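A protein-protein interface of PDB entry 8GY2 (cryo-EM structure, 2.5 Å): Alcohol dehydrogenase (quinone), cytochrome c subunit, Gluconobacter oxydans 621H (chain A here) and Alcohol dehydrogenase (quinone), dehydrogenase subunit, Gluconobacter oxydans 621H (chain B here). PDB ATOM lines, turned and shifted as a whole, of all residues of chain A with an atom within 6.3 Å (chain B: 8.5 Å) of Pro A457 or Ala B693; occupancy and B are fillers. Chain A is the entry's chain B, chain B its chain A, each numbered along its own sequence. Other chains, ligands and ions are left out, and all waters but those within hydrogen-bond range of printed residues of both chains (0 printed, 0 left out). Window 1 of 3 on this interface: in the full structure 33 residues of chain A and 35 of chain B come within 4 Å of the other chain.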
ATOM      1  N   ILE A 381     -21.140  -0.951  23.382  1.00  0.00           N
ATOM      2  CA  ILE A 381     -21.092   0.079  24.410  1.00  0.00           C
ATOM      3  C   ILE A 381     -21.162  -0.595  25.771  1.00  0.00           C
ATOM      4  O   ILE A 381     -22.050  -1.421  26.017  1.00  0.00           O
ATOM      5  CB  ILE A 381     -22.225   1.101  24.226  1.00  0.00           C
ATOM      6  CG1 ILE A 381     -21.987   1.918  22.954  1.00  0.00           C
ATOM      7  CG2 ILE A 381     -22.322   2.009  25.437  1.00  0.00           C
ATOM      8  CD1 ILE A 381     -22.759   1.424  21.751  1.00  0.00           C
ATOM      9  N   ALA A 393     -16.787   2.373  24.342  1.00  0.00           N
ATOM     10  CA  ALA A 393     -17.629   2.170  23.163  1.00  0.00           C
ATOM     11  C   ALA A 393     -16.768   1.760  21.973  1.00  0.00           C
ATOM     12  O   ALA A 393     -16.016   2.583  21.451  1.00  0.00           O
ATOM     13  CB  ALA A 393     -18.413   3.441  22.840  1.00  0.00           C
ATOM     14  N   MET A 394     -16.866   0.506  21.547  1.00  0.00           N
ATOM     15  CA  MET A 394     -16.444   0.135  20.197  1.00  0.00           C
ATOM     16  C   MET A 394     -17.340   0.777  19.152  1.00  0.00           C
ATOM     17  O   MET A 394     -18.562   0.583  19.194  1.00  0.00           O
ATOM     18  CB  MET A 394     -16.493  -1.364  19.985  1.00  0.00           C
ATOM     19  CG  MET A 394     -15.823  -1.883  18.708  1.00  0.00           C
ATOM     20  SD  MET A 394     -14.243  -2.713  18.838  1.00  0.00           S
ATOM     21  CE  MET A 394     -14.210  -3.471  17.208  1.00  0.00           C
ATOM     22  N   TYR A 455     -23.989   4.404  28.599  1.00  0.00           N
ATOM     23  CA  TYR A 455     -24.031   5.738  28.017  1.00  0.00           C
ATOM     24  C   TYR A 455     -23.540   5.709  26.576  1.00  0.00           C
ATOM     25  O   TYR A 455     -22.433   5.240  26.298  1.00  0.00           O
ATOM     26  CB  TYR A 455     -23.191   6.706  28.851  1.00  0.00           C
ATOM     27  CG  TYR A 455     -23.593   6.729  30.307  1.00  0.00           C
ATOM     28  CD1 TYR A 455     -24.831   7.220  30.694  1.00  0.00           C
ATOM     29  CD2 TYR A 455     -22.741   6.252  31.291  1.00  0.00           C
ATOM     30  CE1 TYR A 455     -25.208   7.242  32.019  1.00  0.00           C
ATOM     31  CE2 TYR A 455     -23.111   6.269  32.622  1.00  0.00           C
ATOM     32  CZ  TYR A 455     -24.346   6.764  32.979  1.00  0.00           C
ATOM     33  OH  TYR A 455     -24.722   6.784  34.302  1.00  0.00           O
ATOM     34  N   MET A 456     -24.372   6.212  25.668  1.00  0.00           N
ATOM     35  CA  MET A 456     -24.010   6.259  24.263  1.00  0.00           C
ATOM     36  C   MET A 456     -22.884   7.269  24.039  1.00  0.00           C
ATOM     37  O   MET A 456     -22.808   8.288  24.729  1.00  0.00           O
ATOM     38  CB  MET A 456     -25.223   6.632  23.416  1.00  0.00           C
ATOM     39  CG  MET A 456     -26.306   5.569  23.385  1.00  0.00           C
ATOM     40  SD  MET A 456     -25.637   3.901  23.260  1.00  0.00           S
ATOM     41  CE  MET A 456     -26.065   3.497  21.569  1.00  0.00           C
ATOM     42  N   PRO A 457     -22.001   7.010  23.080  1.00  0.00           N
ATOM     43  CA  PRO A 457     -20.872   7.915  22.859  1.00  0.00           C
ATOM     44  C   PRO A 457     -21.260   9.130  22.032  1.00  0.00           C
ATOM     45  O   PRO A 457     -22.132   9.076  21.163  1.00  0.00           O
ATOM     46  CB  PRO A 457     -19.860   7.042  22.107  1.00  0.00           C
ATOM     47  CG  PRO A 457     -20.660   5.924  21.505  1.00  0.00           C
ATOM     48  CD  PRO A 457     -22.040   5.917  22.095  1.00  0.00           C
ATOM     49  N   GLN A 458     -20.591  10.239  22.324  1.00  0.00           N
ATOM     50  CA  GLN A 458     -20.747  11.449  21.540  1.00  0.00           C
ATOM     51  C   GLN A 458     -20.009  11.314  20.213  1.00  0.00           C
ATOM     52  O   GLN A 458     -19.078  10.516  20.089  1.00  0.00           O
ATOM     53  CB  GLN A 458     -20.216  12.650  22.316  1.00  0.00           C
ATOM     54  CG  GLN A 458     -20.734  12.758  23.739  1.00  0.00           C
ATOM     55  CD  GLN A 458     -22.205  13.109  23.797  1.00  0.00           C
ATOM     56  OE1 GLN A 458     -22.995  12.416  24.436  1.00  0.00           O
ATOM     57  NE2 GLN A 458     -22.582  14.191  23.128  1.00  0.00           N
ATOM     58  N   PRO A 459     -20.418  12.071  19.194  1.00  0.00           N
ATOM     59  CA  PRO A 459     -19.650  12.084  17.944  1.00  0.00           C
ATOM     60  C   PRO A 459     -18.232  12.580  18.182  1.00  0.00           C
ATOM     61  O   PRO A 459     -17.994  13.465  19.005  1.00  0.00           O
ATOM     62  CB  PRO A 459     -20.444  13.040  17.045  1.00  0.00           C
ATOM     63  CG  PRO A 459     -21.369  13.777  17.959  1.00  0.00           C
ATOM     64  CD  PRO A 459     -21.661  12.851  19.088  1.00  0.00           C
ATOM     65  N   TYR A 460     -17.284  11.990  17.452  1.00  0.00           N
ATOM     66  CA  TYR A 460     -15.880  12.340  17.645  1.00  0.00           C
ATOM     67  C   TYR A 460     -15.596  13.766  17.191  1.00  0.00           C
ATOM     68  O   TYR A 460     -14.957  14.540  17.912  1.00  0.00           O
ATOM     69  CB  TYR A 460     -14.988  11.350  16.898  1.00  0.00           C
ATOM     70  CG  TYR A 460     -14.839  10.017  17.590  1.00  0.00           C
ATOM     71  CD1 TYR A 460     -13.865   9.821  18.559  1.00  0.00           C
ATOM     72  CD2 TYR A 460     -15.670   8.953  17.272  1.00  0.00           C
ATOM     73  CE1 TYR A 460     -13.726   8.603  19.192  1.00  0.00           C
ATOM     74  CE2 TYR A 460     -15.538   7.733  17.899  1.00  0.00           C
ATOM     75  CZ  TYR A 460     -14.565   7.563  18.858  1.00  0.00           C
ATOM     76  OH  TYR A 460     -14.432   6.347  19.483  1.00  0.00           O
ATOM     77  N   ARG B  92     -22.808  12.841  34.799  1.00  0.00           N
ATOM     78  CA  ARG B  92     -22.114  14.043  35.240  1.00  0.00           C
ATOM     79  C   ARG B  92     -23.096  14.961  35.968  1.00  0.00           C
ATOM     80  O   ARG B  92     -24.241  14.592  36.240  1.00  0.00           O
ATOM     81  CB  ARG B  92     -21.444  14.744  34.056  1.00  0.00           C
ATOM     82  CG  ARG B  92     -20.833  13.799  33.034  1.00  0.00           C
ATOM     83  CD  ARG B  92     -19.322  13.740  33.168  1.00  0.00           C
ATOM     84  NE  ARG B  92     -18.687  14.990  32.766  1.00  0.00           N
ATOM     85  CZ  ARG B  92     -18.022  15.160  31.632  1.00  0.00           C
ATOM     86  NH1 ARG B  92     -17.885  14.178  30.757  1.00  0.00           N
ATOM     87  NH2 ARG B  92     -17.479  16.345  31.370  1.00  0.00           N
ATOM     88  N   TRP B 111     -24.562  17.213  28.903  1.00  0.00           N
ATOM     89  CA  TRP B 111     -24.335  17.083  27.464  1.00  0.00           C
ATOM     90  C   TRP B 111     -25.424  17.772  26.650  1.00  0.00           C
ATOM     91  O   TRP B 111     -25.660  17.412  25.492  1.00  0.00           O
ATOM     92  CB  TRP B 111     -24.203  15.614  27.042  1.00  0.00           C
ATOM     93  CG  TRP B 111     -22.867  15.013  27.355  1.00  0.00           C
ATOM     94  CD1 TRP B 111     -22.603  14.037  28.268  1.00  0.00           C
ATOM     95  CD2 TRP B 111     -21.612  15.344  26.748  1.00  0.00           C
ATOM     96  NE1 TRP B 111     -21.263  13.742  28.272  1.00  0.00           N
ATOM     97  CE2 TRP B 111     -20.632  14.530  27.347  1.00  0.00           C
ATOM     98  CE3 TRP B 111     -21.222  16.251  25.758  1.00  0.00           C
ATOM     99  CZ2 TRP B 111     -19.288  14.595  26.989  1.00  0.00           C
ATOM    100  CZ3 TRP B 111     -19.888  16.312  25.404  1.00  0.00           C
ATOM    101  CH2 TRP B 111     -18.937  15.490  26.018  1.00  0.00           C
ATOM    102  N   LYS B 113     -28.605  17.709  26.689  1.00  0.00           N
ATOM    103  CA  LYS B 113     -29.785  16.950  26.301  1.00  0.00           C
ATOM    104  C   LYS B 113     -31.032  17.539  26.950  1.00  0.00           C
ATOM    105  O   LYS B 113     -30.982  18.095  28.049  1.00  0.00           O
ATOM    106  CB  LYS B 113     -29.632  15.480  26.689  1.00  0.00           C
ATOM    107  CG  LYS B 113     -28.551  14.751  25.911  1.00  0.00           C
ATOM    108  CD  LYS B 113     -28.312  13.356  26.456  1.00  0.00           C
ATOM    109  CE  LYS B 113     -26.902  12.883  26.149  1.00  0.00           C
ATOM    110  NZ  LYS B 113     -26.808  11.400  26.110  1.00  0.00           N
ATOM    111  N   ASP B 129     -31.575  15.210  21.741  1.00  0.00           N
ATOM    112  CA  ASP B 129     -30.170  15.423  22.047  1.00  0.00           C
ATOM    113  C   ASP B 129     -29.488  16.035  20.830  1.00  0.00           C
ATOM    114  O   ASP B 129     -29.675  15.550  19.700  1.00  0.00           O
ATOM    115  CB  ASP B 129     -29.477  14.119  22.480  1.00  0.00           C
ATOM    116  CG  ASP B 129     -29.188  13.189  21.322  1.00  0.00           C
ATOM    117  OD1 ASP B 129     -30.101  12.949  20.505  1.00  0.00           O
ATOM    118  OD2 ASP B 129     -28.045  12.694  21.232  1.00  0.00           O
ATOM    119  N   LYS B 131     -26.387  16.003  20.042  1.00  0.00           N
ATOM    120  CA  LYS B 131     -25.173  15.269  19.685  1.00  0.00           C
ATOM    121  C   LYS B 131     -23.955  16.194  19.710  1.00  0.00           C
ATOM    122  O   LYS B 131     -23.307  16.450  18.693  1.00  0.00           O
ATOM    123  CB  LYS B 131     -25.328  14.581  18.326  1.00  0.00           C
ATOM    124  CG  LYS B 131     -26.345  13.457  18.326  1.00  0.00           C
ATOM    125  CD  LYS B 131     -26.289  12.655  17.041  1.00  0.00           C
ATOM    126  CE  LYS B 131     -27.669  12.163  16.644  1.00  0.00           C
ATOM    127  NZ  LYS B 131     -28.417  11.617  17.809  1.00  0.00           N
ATOM    128  N   VAL B 132     -23.665  16.703  20.903  1.00  0.00           N
ATOM    129  CA  VAL B 132     -22.514  17.594  21.075  1.00  0.00           C
ATOM    130  C   VAL B 132     -21.235  16.821  20.780  1.00  0.00           C
ATOM    131  O   VAL B 132     -21.028  15.731  21.347  1.00  0.00           O
ATOM    132  CB  VAL B 132     -22.491  18.172  22.501  1.00  0.00           C
ATOM    133  CG1 VAL B 132     -21.167  18.861  22.772  1.00  0.00           C
ATOM    134  CG2 VAL B 132     -23.649  19.134  22.702  1.00  0.00           C
ATOM    135  N   PRO B 133     -20.363  17.314  19.902  1.00  0.00           N
ATOM    136  CA  PRO B 133     -19.121  16.588  19.613  1.00  0.00           C
ATOM    137  C   PRO B 133     -18.268  16.435  20.862  1.00  0.00           C
ATOM    138  O   PRO B 133     -18.199  17.331  21.706  1.00  0.00           O
ATOM    139  CB  PRO B 133     -18.432  17.465  18.562  1.00  0.00           C
ATOM    140  CG  PRO B 133     -19.525  18.297  17.979  1.00  0.00           C
ATOM    141  CD  PRO B 133     -20.491  18.536  19.094  1.00  0.00           C
ATOM    142  N   GLY B 134     -17.614  15.282  20.974  1.00  0.00           N
ATOM    143  CA  GLY B 134     -16.822  14.992  22.152  1.00  0.00           C
ATOM    144  C   GLY B 134     -15.446  15.612  22.177  1.00  0.00           C
ATOM    145  O   GLY B 134     -14.788  15.563  23.220  1.00  0.00           O
ATOM    146  N   ASN B 135     -14.996  16.201  21.072  1.00  0.00           N
ATOM    147  CA  ASN B 135     -13.650  16.749  20.979  1.00  0.00           C
ATOM    148  C   ASN B 135     -13.537  18.166  21.528  1.00  0.00           C
ATOM    149  O   ASN B 135     -12.426  18.703  21.585  1.00  0.00           O
ATOM    150  CB  ASN B 135     -13.168  16.721  19.526  1.00  0.00           C
ATOM    151  CG  ASN B 135     -13.970  17.637  18.629  1.00  0.00           C
ATOM    152  OD1 ASN B 135     -15.194  17.701  18.725  1.00  0.00           O
ATOM    153  ND2 ASN B 135     -13.282  18.351  17.747  1.00  0.00           N
ATOM    154  N   ALA B 137     -15.012  18.887  24.616  1.00  0.00           N
ATOM    155  CA  ALA B 137     -15.365  18.789  26.029  1.00  0.00           C
ATOM    156  C   ALA B 137     -14.310  19.423  26.925  1.00  0.00           C
ATOM    157  O   ALA B 137     -14.635  19.902  28.017  1.00  0.00           O
ATOM    158  CB  ALA B 137     -15.577  17.326  26.415  1.00  0.00           C
ATOM    159  N   GLY B 689      -5.937  10.775  22.458  1.00  0.00           N
ATOM    160  CA  GLY B 689      -7.337  10.957  22.789  1.00  0.00           C
ATOM    161  C   GLY B 689      -8.232   9.810  22.368  1.00  0.00           C
ATOM    162  O   GLY B 689      -9.250  10.024  21.704  1.00  0.00           O
ATOM    163  N   ALA B 690      -7.860   8.583  22.745  1.00  0.00           N
ATOM    164  CA  ALA B 690      -8.635   7.410  22.356  1.00  0.00           C
ATOM    165  C   ALA B 690     -10.062   7.444  22.887  1.00  0.00           C
ATOM    166  O   ALA B 690     -10.942   6.806  22.300  1.00  0.00           O
ATOM    167  CB  ALA B 690      -7.935   6.138  22.837  1.00  0.00           C
ATOM    168  N   LEU B 691     -10.315   8.168  23.975  1.00  0.00           N
ATOM    169  CA  LEU B 691     -11.651   8.283  24.556  1.00  0.00           C
ATOM    170  C   LEU B 691     -12.295   9.626  24.233  1.00  0.00           C
ATOM    171  O   LEU B 691     -12.987  10.211  25.070  1.00  0.00           O
ATOM    172  CB  LEU B 691     -11.594   8.063  26.064  1.00  0.00           C
ATOM    173  CG  LEU B 691     -11.437   6.623  26.549  1.00  0.00           C
ATOM    174  CD1 LEU B 691     -11.320   6.584  28.062  1.00  0.00           C
ATOM    175  CD2 LEU B 691     -12.596   5.763  26.078  1.00  0.00           C
ATOM    176  N   THR B 692     -12.076  10.134  23.017  1.00  0.00           N
ATOM    177  CA  THR B 692     -12.637  11.426  22.634  1.00  0.00           C
ATOM    178  C   THR B 692     -14.158  11.387  22.576  1.00  0.00           C
ATOM    179  O   THR B 692     -14.814  12.414  22.782  1.00  0.00           O
ATOM    180  CB  THR B 692     -12.062  11.864  21.287  1.00  0.00           C
ATOM    181  OG1 THR B 692     -10.637  11.716  21.308  1.00  0.00           O
ATOM    182  CG2 THR B 692     -12.397  13.315  21.004  1.00  0.00           C
ATOM    183  N   ALA B 693     -14.739  10.215  22.319  1.00  0.00           N
ATOM    184  CA  ALA B 693     -16.188  10.094  22.229  1.00  0.00           C
ATOM    185  C   ALA B 693     -16.886  10.319  23.563  1.00  0.00           C
ATOM    186  O   ALA B 693     -18.114  10.452  23.581  1.00  0.00           O
ATOM    187  CB  ALA B 693     -16.568   8.721  21.676  1.00  0.00           C
ATOM    188  N   TYR B 694     -16.147  10.360  24.671  1.00  0.00           N
ATOM    189  CA  TYR B 694     -16.738  10.541  25.986  1.00  0.00           C
ATOM    190  C   TYR B 694     -16.169  11.724  26.757  1.00  0.00           C
ATOM    191  O   TYR B 694     -16.623  11.986  27.876  1.00  0.00           O
ATOM    192  CB  TYR B 694     -16.572   9.265  26.820  1.00  0.00           C
ATOM    193  CG  TYR B 694     -17.525   8.160  26.436  1.00  0.00           C
ATOM    194  CD1 TYR B 694     -18.833   8.155  26.898  1.00  0.00           C
ATOM    195  CD2 TYR B 694     -17.119   7.123  25.611  1.00  0.00           C
ATOM    196  CE1 TYR B 694     -19.708   7.150  26.550  1.00  0.00           C
ATOM    197  CE2 TYR B 694     -17.988   6.112  25.256  1.00  0.00           C
ATOM    198  CZ  TYR B 694     -19.281   6.130  25.729  1.00  0.00           C
ATOM    199  OH  TYR B 694     -20.151   5.125  25.380  1.00  0.00           O
ATOM    200  N   GLY B 695     -15.195  12.443  26.203  1.00  0.00           N
ATOM    201  CA  GLY B 695     -14.694  13.633  26.863  1.00  0.00           C
ATOM    202  C   GLY B 695     -13.190  13.713  27.036  1.00  0.00           C
ATOM    203  O   GLY B 695     -12.666  14.776  27.378  1.00  0.00           O
ATOM    204  N   MET B 696     -12.480  12.608  26.812  1.00  0.00           N
ATOM    205  CA  MET B 696     -11.017  12.605  26.875  1.00  0.00           C
ATOM    206  C   MET B 696     -10.458  13.010  25.521  1.00  0.00           C
ATOM    207  O   MET B 696     -10.376  12.198  24.599  1.00  0.00           O
ATOM    208  CB  MET B 696     -10.483  11.242  27.293  1.00  0.00           C
ATOM    209  CG  MET B 696      -9.786  11.267  28.626  1.00  0.00           C
ATOM    210  SD  MET B 696      -8.725  12.716  28.778  1.00  0.00           S
ATOM    211  CE  MET B 696      -7.182  12.086  28.136  1.00  0.00           C
ATOM    212  N   ASP B 697     -10.040  14.263  25.411  1.00  0.00           N
ATOM    213  CA  ASP B 697      -9.492  14.781  24.171  1.00  0.00           C
ATOM    214  C   ASP B 697      -7.974  14.659  24.164  1.00  0.00           C
ATOM    215  O   ASP B 697      -7.333  14.478  25.200  1.00  0.00           O
ATOM    216  CB  ASP B 697      -9.920  16.233  23.979  1.00  0.00           C
ATOM    217  CG  ASP B 697     -11.411  16.412  24.136  1.00  0.00           C
ATOM    218  OD1 ASP B 697     -12.154  15.523  23.680  1.00  0.00           O
ATOM    219  OD2 ASP B 697     -11.842  17.423  24.724  1.00  0.00           O
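The backbone carbonyl oxygen (O) of Val B132 is in hydrogen-bond range of the side-chain amide nitrogen (NE2) of Gln A458 (2.8 Å).
N of Gly B134 is in hydrogen-bond range of O of Pro A459 (2.7 Å).
The side-chain amide oxygen of Asn B135 lies close to the backbone carbonyl oxygen of Tyr A460, at 3.3 Å.
The backbone carbonyl oxygen of Ala B693 sits at hydrogen-bond distance from the backbone NH of Gln A458 (2.8 Å).
The side-chain hydroxyl (OH) of Tyr B694 sits at hydrogen-bond distance from the backbone carbonyl oxygen (O) of Tyr A455 (2.5 Å).
The side-chain amino group (NZ) of Lys B131 lies within salt-bridge range of the side-chain carboxylate (OD1) of Asp B129, 3.4 Å away.
The backbone carbonyl oxygen of Gly B134 lies close to the side-chain carboxylate of Asp B697 (2.7 Å).
The side-chain hydroxyl (OG1) of Thr B692 lies close to the backbone carbonyl oxygen (O) of Met B696, at 3.3 Å.
Among the printed residues, merely in contact across the chains: Pro A459 with Pro B133, Pro A459 with Lys B131, Pro A457 with Tyr B694, Ala A393 with Tyr B694, Gln A458 with Trp B111, Tyr A460 with Ala B693, Pro A459 with Val B132, Pro A457 with Ala B693, Met A456 with Tyr B694, Ile A381 with Tyr B694, Tyr A460 with Thr B692 and Gln A458 with Gly B134.
Of chain A, only Pro A457, Gln A458 and Tyr A460 come within 4 Å of Ala B693.
Printed residues of chain A within 4 Å of Thr B692: Tyr A460.
Of the printed residues of chain A, Val B132 touches Gln A458 (2.8 Å) and Pro A459 (3.7 Å).
Of the printed residues of chain B, Ile A381 touches Tyr B694.
Printed residues of chain A within 4 Å of Pro B133: Pro A459 (3.4 Å).
Gly B689 touches none of the printed residues of chain A.
Gly B695 touches none of the printed residues of chain A.
The nearest residue of chain A that does not touch Ala B693 is Pro A459 (5.0 Å).
Of the 9 printed residues of chain A, 8 touch a printed residue of chain B.
Hydrophobic or aromatic side chains of chain A that line the printed part of chain B: Ile A381, Ala A393, Pro A457, Pro A459 and Tyr A460.
Among the printed residues, no Asp or Glu carboxylate lies within 4 Å of a Lys or Arg side-chain nitrogen of the other chain.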
